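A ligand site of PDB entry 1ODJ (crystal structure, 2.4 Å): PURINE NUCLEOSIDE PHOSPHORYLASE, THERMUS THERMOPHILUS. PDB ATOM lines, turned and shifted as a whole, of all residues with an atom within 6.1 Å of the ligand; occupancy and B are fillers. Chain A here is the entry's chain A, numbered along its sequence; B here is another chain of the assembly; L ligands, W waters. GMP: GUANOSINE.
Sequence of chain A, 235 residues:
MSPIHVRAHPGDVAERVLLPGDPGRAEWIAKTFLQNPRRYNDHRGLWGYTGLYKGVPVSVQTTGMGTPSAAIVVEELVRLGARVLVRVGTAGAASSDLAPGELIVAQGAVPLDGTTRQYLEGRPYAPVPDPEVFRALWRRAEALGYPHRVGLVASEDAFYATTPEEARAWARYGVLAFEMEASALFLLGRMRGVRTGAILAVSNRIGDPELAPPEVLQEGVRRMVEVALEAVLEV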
ATOM      1  N   GLY A  21      -6.508   0.617  13.328  1.00  0.00           N
ATOM      2  CA  GLY A  21      -5.647  -0.554  13.198  1.00  0.00           C
ATOM      3  C   GLY A  21      -5.747  -1.291  11.859  1.00  0.00           C
ATOM      4  O   GLY A  21      -4.752  -1.770  11.328  1.00  0.00           O
ATOM      5  N   GLY A  64      -1.570  -1.200  12.177  1.00  0.00           N
ATOM      6  CA  GLY A  64      -1.321  -2.631  12.116  1.00  0.00           C
ATOM      7  C   GLY A  64      -1.771  -3.178  13.454  1.00  0.00           C
ATOM      8  O   GLY A  64      -2.205  -2.401  14.306  1.00  0.00           O
ATOM      9  N   MET A  65      -1.685  -4.489  13.654  1.00  0.00           N
ATOM     10  CA  MET A  65      -2.095  -5.077  14.927  1.00  0.00           C
ATOM     11  C   MET A  65      -0.892  -5.275  15.840  1.00  0.00           C
ATOM     12  O   MET A  65       0.112  -5.865  15.447  1.00  0.00           O
ATOM     13  CB  MET A  65      -2.805  -6.419  14.707  1.00  0.00           C
ATOM     14  CG  MET A  65      -4.130  -6.311  13.967  1.00  0.00           C
ATOM     15  SD  MET A  65      -5.096  -7.838  13.984  1.00  0.00           S
ATOM     16  CE  MET A  65      -4.233  -8.753  12.724  1.00  0.00           C
ATOM     17  N   GLY A  66      -0.990  -4.768  17.073  1.00  0.00           N
ATOM     18  CA  GLY A  66       0.105  -4.914  18.016  1.00  0.00           C
ATOM     19  C   GLY A  66       0.919  -3.653  18.257  1.00  0.00           C
ATOM     20  O   GLY A  66       1.114  -2.820  17.361  1.00  0.00           O
ATOM     21  N   ARG A  87      -5.953   7.267  18.361  1.00  0.00           N
ATOM     22  CA  ARG A  87      -6.196   5.904  17.920  1.00  0.00           C
ATOM     23  C   ARG A  87      -7.699   5.695  17.862  1.00  0.00           C
ATOM     24  O   ARG A  87      -8.404   6.026  18.813  1.00  0.00           O
ATOM     25  CB  ARG A  87      -5.588   4.896  18.912  1.00  0.00           C
ATOM     26  CG  ARG A  87      -5.914   3.440  18.572  1.00  0.00           C
ATOM     27  CD  ARG A  87      -5.182   2.445  19.484  1.00  0.00           C
ATOM     28  NE  ARG A  87      -6.059   1.349  19.851  1.00  0.00           N
ATOM     29  CZ  ARG A  87      -6.531   0.456  18.988  1.00  0.00           C
ATOM     30  NH1 ARG A  87      -6.205   0.522  17.709  1.00  0.00           N
ATOM     31  NH2 ARG A  87      -7.389  -0.475  19.400  1.00  0.00           N
ATOM     32  N   THR A  90     -11.049  -0.897  17.745  1.00  0.00           N
ATOM     33  CA  THR A  90     -12.032  -1.768  18.385  1.00  0.00           C
ATOM     34  C   THR A  90     -11.435  -2.462  19.587  1.00  0.00           C
ATOM     35  O   THR A  90     -10.224  -2.418  19.785  1.00  0.00           O
ATOM     36  CB  THR A  90     -12.518  -2.839  17.420  1.00  0.00           C
ATOM     37  OG1 THR A  90     -11.388  -3.585  16.968  1.00  0.00           O
ATOM     38  CG2 THR A  90     -13.213  -2.207  16.247  1.00  0.00           C
ATOM     39  N   ALA A  91     -12.270  -3.131  20.381  1.00  0.00           N
ATOM     40  CA  ALA A  91     -11.782  -3.817  21.562  1.00  0.00           C
ATOM     41  C   ALA A  91     -12.736  -4.868  22.111  1.00  0.00           C
ATOM     42  O   ALA A  91     -13.942  -4.779  21.935  1.00  0.00           O
ATOM     43  CB  ALA A  91     -11.441  -2.787  22.659  1.00  0.00           C
ATOM     44  N   GLY A  92     -12.178  -5.869  22.791  1.00  0.00           N
ATOM     45  CA  GLY A  92     -12.989  -6.923  23.371  1.00  0.00           C
ATOM     46  C   GLY A  92     -13.329  -6.584  24.816  1.00  0.00           C
ATOM     47  O   GLY A  92     -12.423  -6.434  25.620  1.00  0.00           O
ATOM     48  N   ALA A  93     -14.615  -6.478  25.126  1.00  0.00           N
ATOM     49  CA  ALA A  93     -15.077  -6.149  26.481  1.00  0.00           C
ATOM     50  C   ALA A  93     -14.600  -7.140  27.543  1.00  0.00           C
ATOM     51  O   ALA A  93     -14.626  -8.353  27.331  1.00  0.00           O
ATOM     52  CB  ALA A  93     -16.597  -6.083  26.488  1.00  0.00           C
ATOM     53  N   ALA A 154      -6.872  -2.562  28.445  1.00  0.00           N
ATOM     54  CA  ALA A 154      -5.602  -3.233  28.662  1.00  0.00           C
ATOM     55  C   ALA A 154      -4.993  -3.568  27.316  1.00  0.00           C
ATOM     56  O   ALA A 154      -5.686  -4.052  26.417  1.00  0.00           O
ATOM     57  CB  ALA A 154      -5.797  -4.488  29.509  1.00  0.00           C
ATOM     58  N   GLU A 156      -2.624  -5.895  25.344  1.00  0.00           N
ATOM     59  CA  GLU A 156      -1.864  -7.136  25.400  1.00  0.00           C
ATOM     60  C   GLU A 156      -1.161  -7.437  24.075  1.00  0.00           C
ATOM     61  O   GLU A 156      -1.347  -6.731  23.083  1.00  0.00           O
ATOM     62  CB  GLU A 156      -2.762  -8.317  25.812  1.00  0.00           C
ATOM     63  CG  GLU A 156      -3.984  -8.545  24.930  1.00  0.00           C
ATOM     64  CD  GLU A 156      -4.805  -9.754  25.391  1.00  0.00           C
ATOM     65  OE1 GLU A 156      -5.847 -10.030  24.770  1.00  0.00           O
ATOM     66  OE2 GLU A 156      -4.416 -10.421  26.383  1.00  0.00           O
ATOM     67  N   ALA A 158      -0.570 -11.123  23.059  1.00  0.00           N
ATOM     68  CA  ALA A 158      -1.117 -12.377  22.584  1.00  0.00           C
ATOM     69  C   ALA A 158      -2.623 -12.409  22.630  1.00  0.00           C
ATOM     70  O   ALA A 158      -3.219 -12.687  23.667  1.00  0.00           O
ATOM     71  CB  ALA A 158      -0.560 -13.521  23.415  1.00  0.00           C
ATOM     72  N   PHE A 159      -3.231 -12.128  21.476  1.00  0.00           N
ATOM     73  CA  PHE A 159      -4.690 -12.102  21.316  1.00  0.00           C
ATOM     74  C   PHE A 159      -5.324 -13.383  21.855  1.00  0.00           C
ATOM     75  O   PHE A 159      -6.241 -13.329  22.675  1.00  0.00           O
ATOM     76  CB  PHE A 159      -5.009 -11.950  19.829  1.00  0.00           C
ATOM     77  CG  PHE A 159      -6.461 -11.741  19.539  1.00  0.00           C
ATOM     78  CD1 PHE A 159      -7.018 -10.461  19.574  1.00  0.00           C
ATOM     79  CD2 PHE A 159      -7.277 -12.809  19.187  1.00  0.00           C
ATOM     80  CE1 PHE A 159      -8.366 -10.249  19.271  1.00  0.00           C
ATOM     81  CE2 PHE A 159      -8.627 -12.603  18.871  1.00  0.00           C
ATOM     82  CZ  PHE A 159      -9.171 -11.323  18.913  1.00  0.00           C
ATOM     83  N   PHE A 178     -10.060  -5.149  26.283  1.00  0.00           N
ATOM     84  CA  PHE A 178      -8.735  -5.471  25.780  1.00  0.00           C
ATOM     85  C   PHE A 178      -8.539  -5.040  24.335  1.00  0.00           C
ATOM     86  O   PHE A 178      -9.466  -5.145  23.514  1.00  0.00           O
ATOM     87  CB  PHE A 178      -8.455  -6.981  25.940  1.00  0.00           C
ATOM     88  CG  PHE A 178      -8.233  -7.426  27.367  1.00  0.00           C
ATOM     89  CD1 PHE A 178      -9.269  -7.410  28.301  1.00  0.00           C
ATOM     90  CD2 PHE A 178      -6.981  -7.861  27.781  1.00  0.00           C
ATOM     91  CE1 PHE A 178      -9.066  -7.806  29.633  1.00  0.00           C
ATOM     92  CE2 PHE A 178      -6.768  -8.263  29.106  1.00  0.00           C
ATOM     93  CZ  PHE A 178      -7.822  -8.239  30.032  1.00  0.00           C
ATOM     94  N   GLU A 179      -7.338  -4.550  24.042  1.00  0.00           N
ATOM     95  CA  GLU A 179      -6.937  -4.111  22.708  1.00  0.00           C
ATOM     96  C   GLU A 179      -5.421  -4.313  22.542  1.00  0.00           C
ATOM     97  O   GLU A 179      -4.777  -4.868  23.413  1.00  0.00           O
ATOM     98  CB  GLU A 179      -7.372  -2.654  22.457  1.00  0.00           C
ATOM     99  CG  GLU A 179      -6.998  -1.615  23.494  1.00  0.00           C
ATOM    100  CD  GLU A 179      -5.710  -0.883  23.169  1.00  0.00           C
ATOM    101  OE1 GLU A 179      -4.675  -1.213  23.779  1.00  0.00           O
ATOM    102  OE2 GLU A 179      -5.736   0.009  22.289  1.00  0.00           O
ATOM    103  N   MET A 180      -4.859  -3.873  21.420  1.00  0.00           N
ATOM    104  CA  MET A 180      -3.438  -4.095  21.189  1.00  0.00           C
ATOM    105  C   MET A 180      -2.583  -2.948  20.657  1.00  0.00           C
ATOM    106  O   MET A 180      -1.695  -3.175  19.842  1.00  0.00           O
ATOM    107  CB  MET A 180      -3.264  -5.312  20.248  1.00  0.00           C
ATOM    108  CG  MET A 180      -3.592  -6.662  20.895  1.00  0.00           C
ATOM    109  SD  MET A 180      -3.845  -8.078  19.754  1.00  0.00           S
ATOM    110  CE  MET A 180      -2.194  -8.166  18.934  1.00  0.00           C
ATOM    111  N   GLU A 181      -2.850  -1.712  21.093  1.00  0.00           N
ATOM    112  CA  GLU A 181      -2.050  -0.575  20.634  1.00  0.00           C
ATOM    113  C   GLU A 181      -1.917   0.586  21.593  1.00  0.00           C
ATOM    114  O   GLU A 181      -0.838   1.177  21.696  1.00  0.00           O
ATOM    115  CB  GLU A 181      -2.581  -0.022  19.320  1.00  0.00           C
ATOM    116  CG  GLU A 181      -2.291  -0.890  18.138  1.00  0.00           C
ATOM    117  CD  GLU A 181      -3.314  -1.975  17.993  1.00  0.00           C
ATOM    118  OE1 GLU A 181      -3.037  -2.965  17.278  1.00  0.00           O
ATOM    119  OE2 GLU A 181      -4.396  -1.806  18.593  1.00  0.00           O
ATOM    120  N   LEU A 200     -12.555   3.829  21.544  1.00  0.00           N
ATOM    121  CA  LEU A 200     -12.813   2.484  21.028  1.00  0.00           C
ATOM    122  C   LEU A 200     -14.255   2.043  20.889  1.00  0.00           C
ATOM    123  O   LEU A 200     -15.122   2.416  21.680  1.00  0.00           O
ATOM    124  CB  LEU A 200     -12.064   1.460  21.887  1.00  0.00           C
ATOM    125  CG  LEU A 200     -10.575   1.812  22.050  1.00  0.00           C
ATOM    126  CD1 LEU A 200     -10.218   1.933  23.528  1.00  0.00           C
ATOM    127  CD2 LEU A 200      -9.739   0.772  21.330  1.00  0.00           C
ATOM    128  N   SER A 203     -16.258  -4.450  20.079  1.00  0.00           N
ATOM    129  CA  SER A 203     -16.636  -5.347  18.991  1.00  0.00           C
ATOM    130  C   SER A 203     -17.149  -6.709  19.458  1.00  0.00           C
ATOM    131  O   SER A 203     -17.687  -7.476  18.658  1.00  0.00           O
ATOM    132  CB  SER A 203     -15.461  -5.527  18.017  1.00  0.00           C
ATOM    133  OG  SER A 203     -14.375  -6.191  18.628  1.00  0.00           O
ATOM    134  N   ASN A 204     -16.985  -7.006  20.738  1.00  0.00           N
ATOM    135  CA  ASN A 204     -17.443  -8.280  21.292  1.00  0.00           C
ATOM    136  C   ASN A 204     -17.038  -8.463  22.751  1.00  0.00           C
ATOM    137  O   ASN A 204     -16.212  -7.720  23.290  1.00  0.00           O
ATOM    138  CB  ASN A 204     -16.864  -9.446  20.484  1.00  0.00           C
ATOM    139  CG  ASN A 204     -15.350  -9.477  20.524  1.00  0.00           C
ATOM    140  OD1 ASN A 204     -14.689  -9.026  19.594  1.00  0.00           O
ATOM    141  ND2 ASN A 204     -14.796  -9.985  21.617  1.00  0.00           N
ATOM    142  N   ILE A 206     -15.271 -10.829  25.564  1.00  0.00           N
ATOM    143  CA  ILE A 206     -14.245 -11.873  25.608  1.00  0.00           C
ATOM    144  C   ILE A 206     -14.840 -13.259  25.878  1.00  0.00           C
ATOM    145  O   ILE A 206     -15.498 -13.478  26.889  1.00  0.00           O
ATOM    146  CB  ILE A 206     -13.193 -11.552  26.687  1.00  0.00           C
ATOM    147  CG1 ILE A 206     -12.439 -10.278  26.314  1.00  0.00           C
ATOM    148  CG2 ILE A 206     -12.237 -12.713  26.848  1.00  0.00           C
ATOM    149  CD1 ILE A 206     -11.642 -10.392  25.032  1.00  0.00           C
ATOM    150  N   LEU A 211     -17.667 -12.022  16.377  1.00  0.00           N
ATOM    151  CA  LEU A 211     -18.176 -10.729  16.840  1.00  0.00           C
ATOM    152  C   LEU A 211     -19.721 -10.686  16.967  1.00  0.00           C
ATOM    153  O   LEU A 211     -20.384 -11.729  16.919  1.00  0.00           O
ATOM    154  CB  LEU A 211     -17.663  -9.608  15.904  1.00  0.00           C
ATOM    155  CG  LEU A 211     -16.186  -9.630  15.469  1.00  0.00           C
ATOM    156  CD1 LEU A 211     -15.862  -8.354  14.683  1.00  0.00           C
ATOM    157  CD2 LEU A 211     -15.263  -9.749  16.666  1.00  0.00           C
ATOM    158  N   ILE B   4     -11.208 -15.172  12.703  1.00  0.00           N
ATOM    159  CA  ILE B   4     -11.453 -13.752  12.845  1.00  0.00           C
ATOM    160  C   ILE B   4     -10.653 -12.830  11.920  1.00  0.00           C
ATOM    161  O   ILE B   4     -11.212 -11.922  11.295  1.00  0.00           O
ATOM    162  CB  ILE B   4     -11.231 -13.322  14.296  1.00  0.00           C
ATOM    163  CG1 ILE B   4     -12.300 -13.977  15.172  1.00  0.00           C
ATOM    164  CG2 ILE B   4     -11.259 -11.818  14.418  1.00  0.00           C
ATOM    165  CD1 ILE B   4     -12.277 -13.541  16.620  1.00  0.00           C
ATOM    166  N   HIS B   5      -9.351 -13.063  11.807  1.00  0.00           N
ATOM    167  CA  HIS B   5      -8.513 -12.211  10.984  1.00  0.00           C
ATOM    168  C   HIS B   5      -8.210 -12.780   9.599  1.00  0.00           C
ATOM    169  O   HIS B   5      -8.600 -12.173   8.586  1.00  0.00           O
ATOM    170  CB  HIS B   5      -7.223 -11.899  11.731  1.00  0.00           C
ATOM    171  CG  HIS B   5      -7.453 -11.401  13.121  1.00  0.00           C
ATOM    172  ND1 HIS B   5      -7.924 -12.204  14.136  1.00  0.00           N
ATOM    173  CD2 HIS B   5      -7.287 -10.168  13.663  1.00  0.00           C
ATOM    174  CE1 HIS B   5      -8.033 -11.488  15.245  1.00  0.00           C
ATOM    175  NE2 HIS B   5      -7.653 -10.255  14.986  1.00  0.00           N
ATOM    176  N   ARG B  44      -7.822  -6.846   6.571  1.00  0.00           N
ATOM    177  CA  ARG B  44      -6.738  -6.278   7.360  1.00  0.00           C
ATOM    178  C   ARG B  44      -5.380  -6.234   6.641  1.00  0.00           C
ATOM    179  O   ARG B  44      -4.322  -6.210   7.280  1.00  0.00           O
ATOM    180  CB  ARG B  44      -6.609  -7.042   8.668  1.00  0.00           C
ATOM    181  CG  ARG B  44      -7.632  -6.619   9.702  1.00  0.00           C
ATOM    182  CD  ARG B  44      -7.558  -7.514  10.916  1.00  0.00           C
ATOM    183  NE  ARG B  44      -8.384  -7.039  12.006  1.00  0.00           N
ATOM    184  CZ  ARG B  44      -8.143  -5.925  12.696  1.00  0.00           C
ATOM    185  NH1 ARG B  44      -7.091  -5.172  12.397  1.00  0.00           N
ATOM    186  NH2 ARG B  44      -8.920  -5.591  13.723  1.00  0.00           N
ATOM    187  N   ILE B  72      -1.383 -14.189  15.833  1.00  0.00           N
ATOM    188  CA  ILE B  72      -2.766 -14.270  15.423  1.00  0.00           C
ATOM    189  C   ILE B  72      -2.836 -15.007  14.090  1.00  0.00           C
ATOM    190  O   ILE B  72      -3.664 -15.907  13.916  1.00  0.00           O
ATOM    191  CB  ILE B  72      -3.364 -12.875  15.247  1.00  0.00           C
ATOM    192  CG1 ILE B  72      -3.645 -12.262  16.626  1.00  0.00           C
ATOM    193  CG2 ILE B  72      -4.611 -12.970  14.382  1.00  0.00           C
ATOM    194  CD1 ILE B  72      -3.957 -10.801  16.567  1.00  0.00           C
HETATM  195  O5' GMP L   1      -8.627  -8.075  16.175  1.00  0.00           O
HETATM  196  C5' GMP L   1      -7.606  -7.763  17.099  1.00  0.00           C
HETATM  197  C4' GMP L   1      -7.370  -6.265  16.870  1.00  0.00           C
HETATM  198  O4' GMP L   1      -8.531  -5.402  17.139  1.00  0.00           O
HETATM  199  C3' GMP L   1      -6.283  -5.699  17.774  1.00  0.00           C
HETATM  200  O3' GMP L   1      -5.502  -4.808  16.926  1.00  0.00           O
HETATM  201  C2' GMP L   1      -7.008  -4.907  18.907  1.00  0.00           C
HETATM  202  O2' GMP L   1      -6.531  -3.581  19.114  1.00  0.00           O
HETATM  203  C1' GMP L   1      -8.511  -5.052  18.538  1.00  0.00           C
HETATM  204  N9  GMP L   1      -9.313  -6.000  19.389  1.00  0.00           N
HETATM  205  C8  GMP L   1     -10.675  -6.178  19.263  1.00  0.00           C
HETATM  206  N7  GMP L   1     -11.159  -7.043  20.114  1.00  0.00           N
HETATM  207  C5  GMP L   1     -10.065  -7.474  20.843  1.00  0.00           C
HETATM  208  C6  GMP L   1      -9.992  -8.433  21.899  1.00  0.00           C
HETATM  209  O6  GMP L   1     -10.903  -9.093  22.413  1.00  0.00           O
HETATM  210  N1  GMP L   1      -8.695  -8.582  22.367  1.00  0.00           N
HETATM  211  C2  GMP L   1      -7.599  -7.903  21.885  1.00  0.00           C
HETATM  212  N2  GMP L   1      -6.433  -8.207  22.478  1.00  0.00           N
HETATM  213  N3  GMP L   1      -7.650  -7.011  20.901  1.00  0.00           N
HETATM  214  C4  GMP L   1      -8.909  -6.845  20.422  1.00  0.00           C
HETATM  215  O   HOH W   1      -8.216 -10.401  24.362  1.00  0.00           O
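A ring nitrogen (NE2) of His 5 of chain B is in hydrogen-bond range of an oxygen (O5') of the ligand, at 2.7 Å.
OE2 of Glu 181 lies within hydrogen-bond range of O2' of the ligand, 2.8 Å away.
N of Met 180 lies within hydrogen-bond range of O2' of the ligand, at 2.9 Å.
The side-chain sulfur of Met 180 lies close to a nitrogen (N2) of the ligand.
A nitrogen (N2) of the ligand is in hydrogen-bond range of the side-chain carboxylate of Glu 156 (3.0 Å).
A nitrogen (N7) of the ligand is in hydrogen-bond range of the backbone NH of Gly 92.
O2' of the ligand is in hydrogen-bond range of NH2 of Arg 87.
An oxygen (O4') of the ligand sits at hydrogen-bond distance from the side-chain hydroxyl of Thr 90, 3.4 Å away.
An oxygen (O4') of the ligand lies within hydrogen-bond range of the guanidinium group of Arg 44 of chain B, 3.4 Å away.
The side-chain carboxylate (OE2) of Glu 181 is in salt-bridge range of the guanidinium group (NH1) of Arg 87 (3.1 Å).
N of Glu 181 sits at hydrogen-bond distance from OE1 of Glu 179 (3.3 Å).
The side-chain carboxylate (OE1) of Glu 181 lies within hydrogen-bond range of the backbone NH (N) of Gly 66 (2.7 Å).
The backbone carbonyl oxygen (O) of Met 180 sits close to the backbone NH (N) of Gly 66.
The backbone NH (N) of Phe 178 lies within hydrogen-bond range of the backbone carbonyl oxygen (O) of Gly 92 (2.8 Å).
The backbone NH of Ser 203 sits at hydrogen-bond distance from the backbone carbonyl oxygen of Ala 91, at 3.0 Å.
NH1 of Arg 44 of chain B lies close to SD of Met 65 (3.7 Å).
The side-chain amide oxygen (OD1) of Asn 204 is in hydrogen-bond range of the side-chain hydroxyl (OG) of Ser 203 (3.0 Å).
Met 65 touches the ligand (CG to O3', 3.6 Å).
Ala 91 touches the ligand.
Phe 159 touches the ligand (CE1 to C5', 3.4 Å).
Phe 178 touches the ligand (O to C4, 3.6 Å).
Glu 179 touches the ligand (CA to N3, 3.5 Å).
OG of Ser 203 touches N7 of the ligand, at 3.6 Å.
Ile 206 touches the ligand.
Hydrophobic or aromatic side chains that line the ligand: Met 65, Phe 159, Phe 178, Met 180, Ile 206 and His 5 of chain B.
The nearest printed residue that does not touch the ligand is Asn 204 (4.1 Å).
Water W1 bridges OE1 of Glu 156 and N1 of the ligand.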
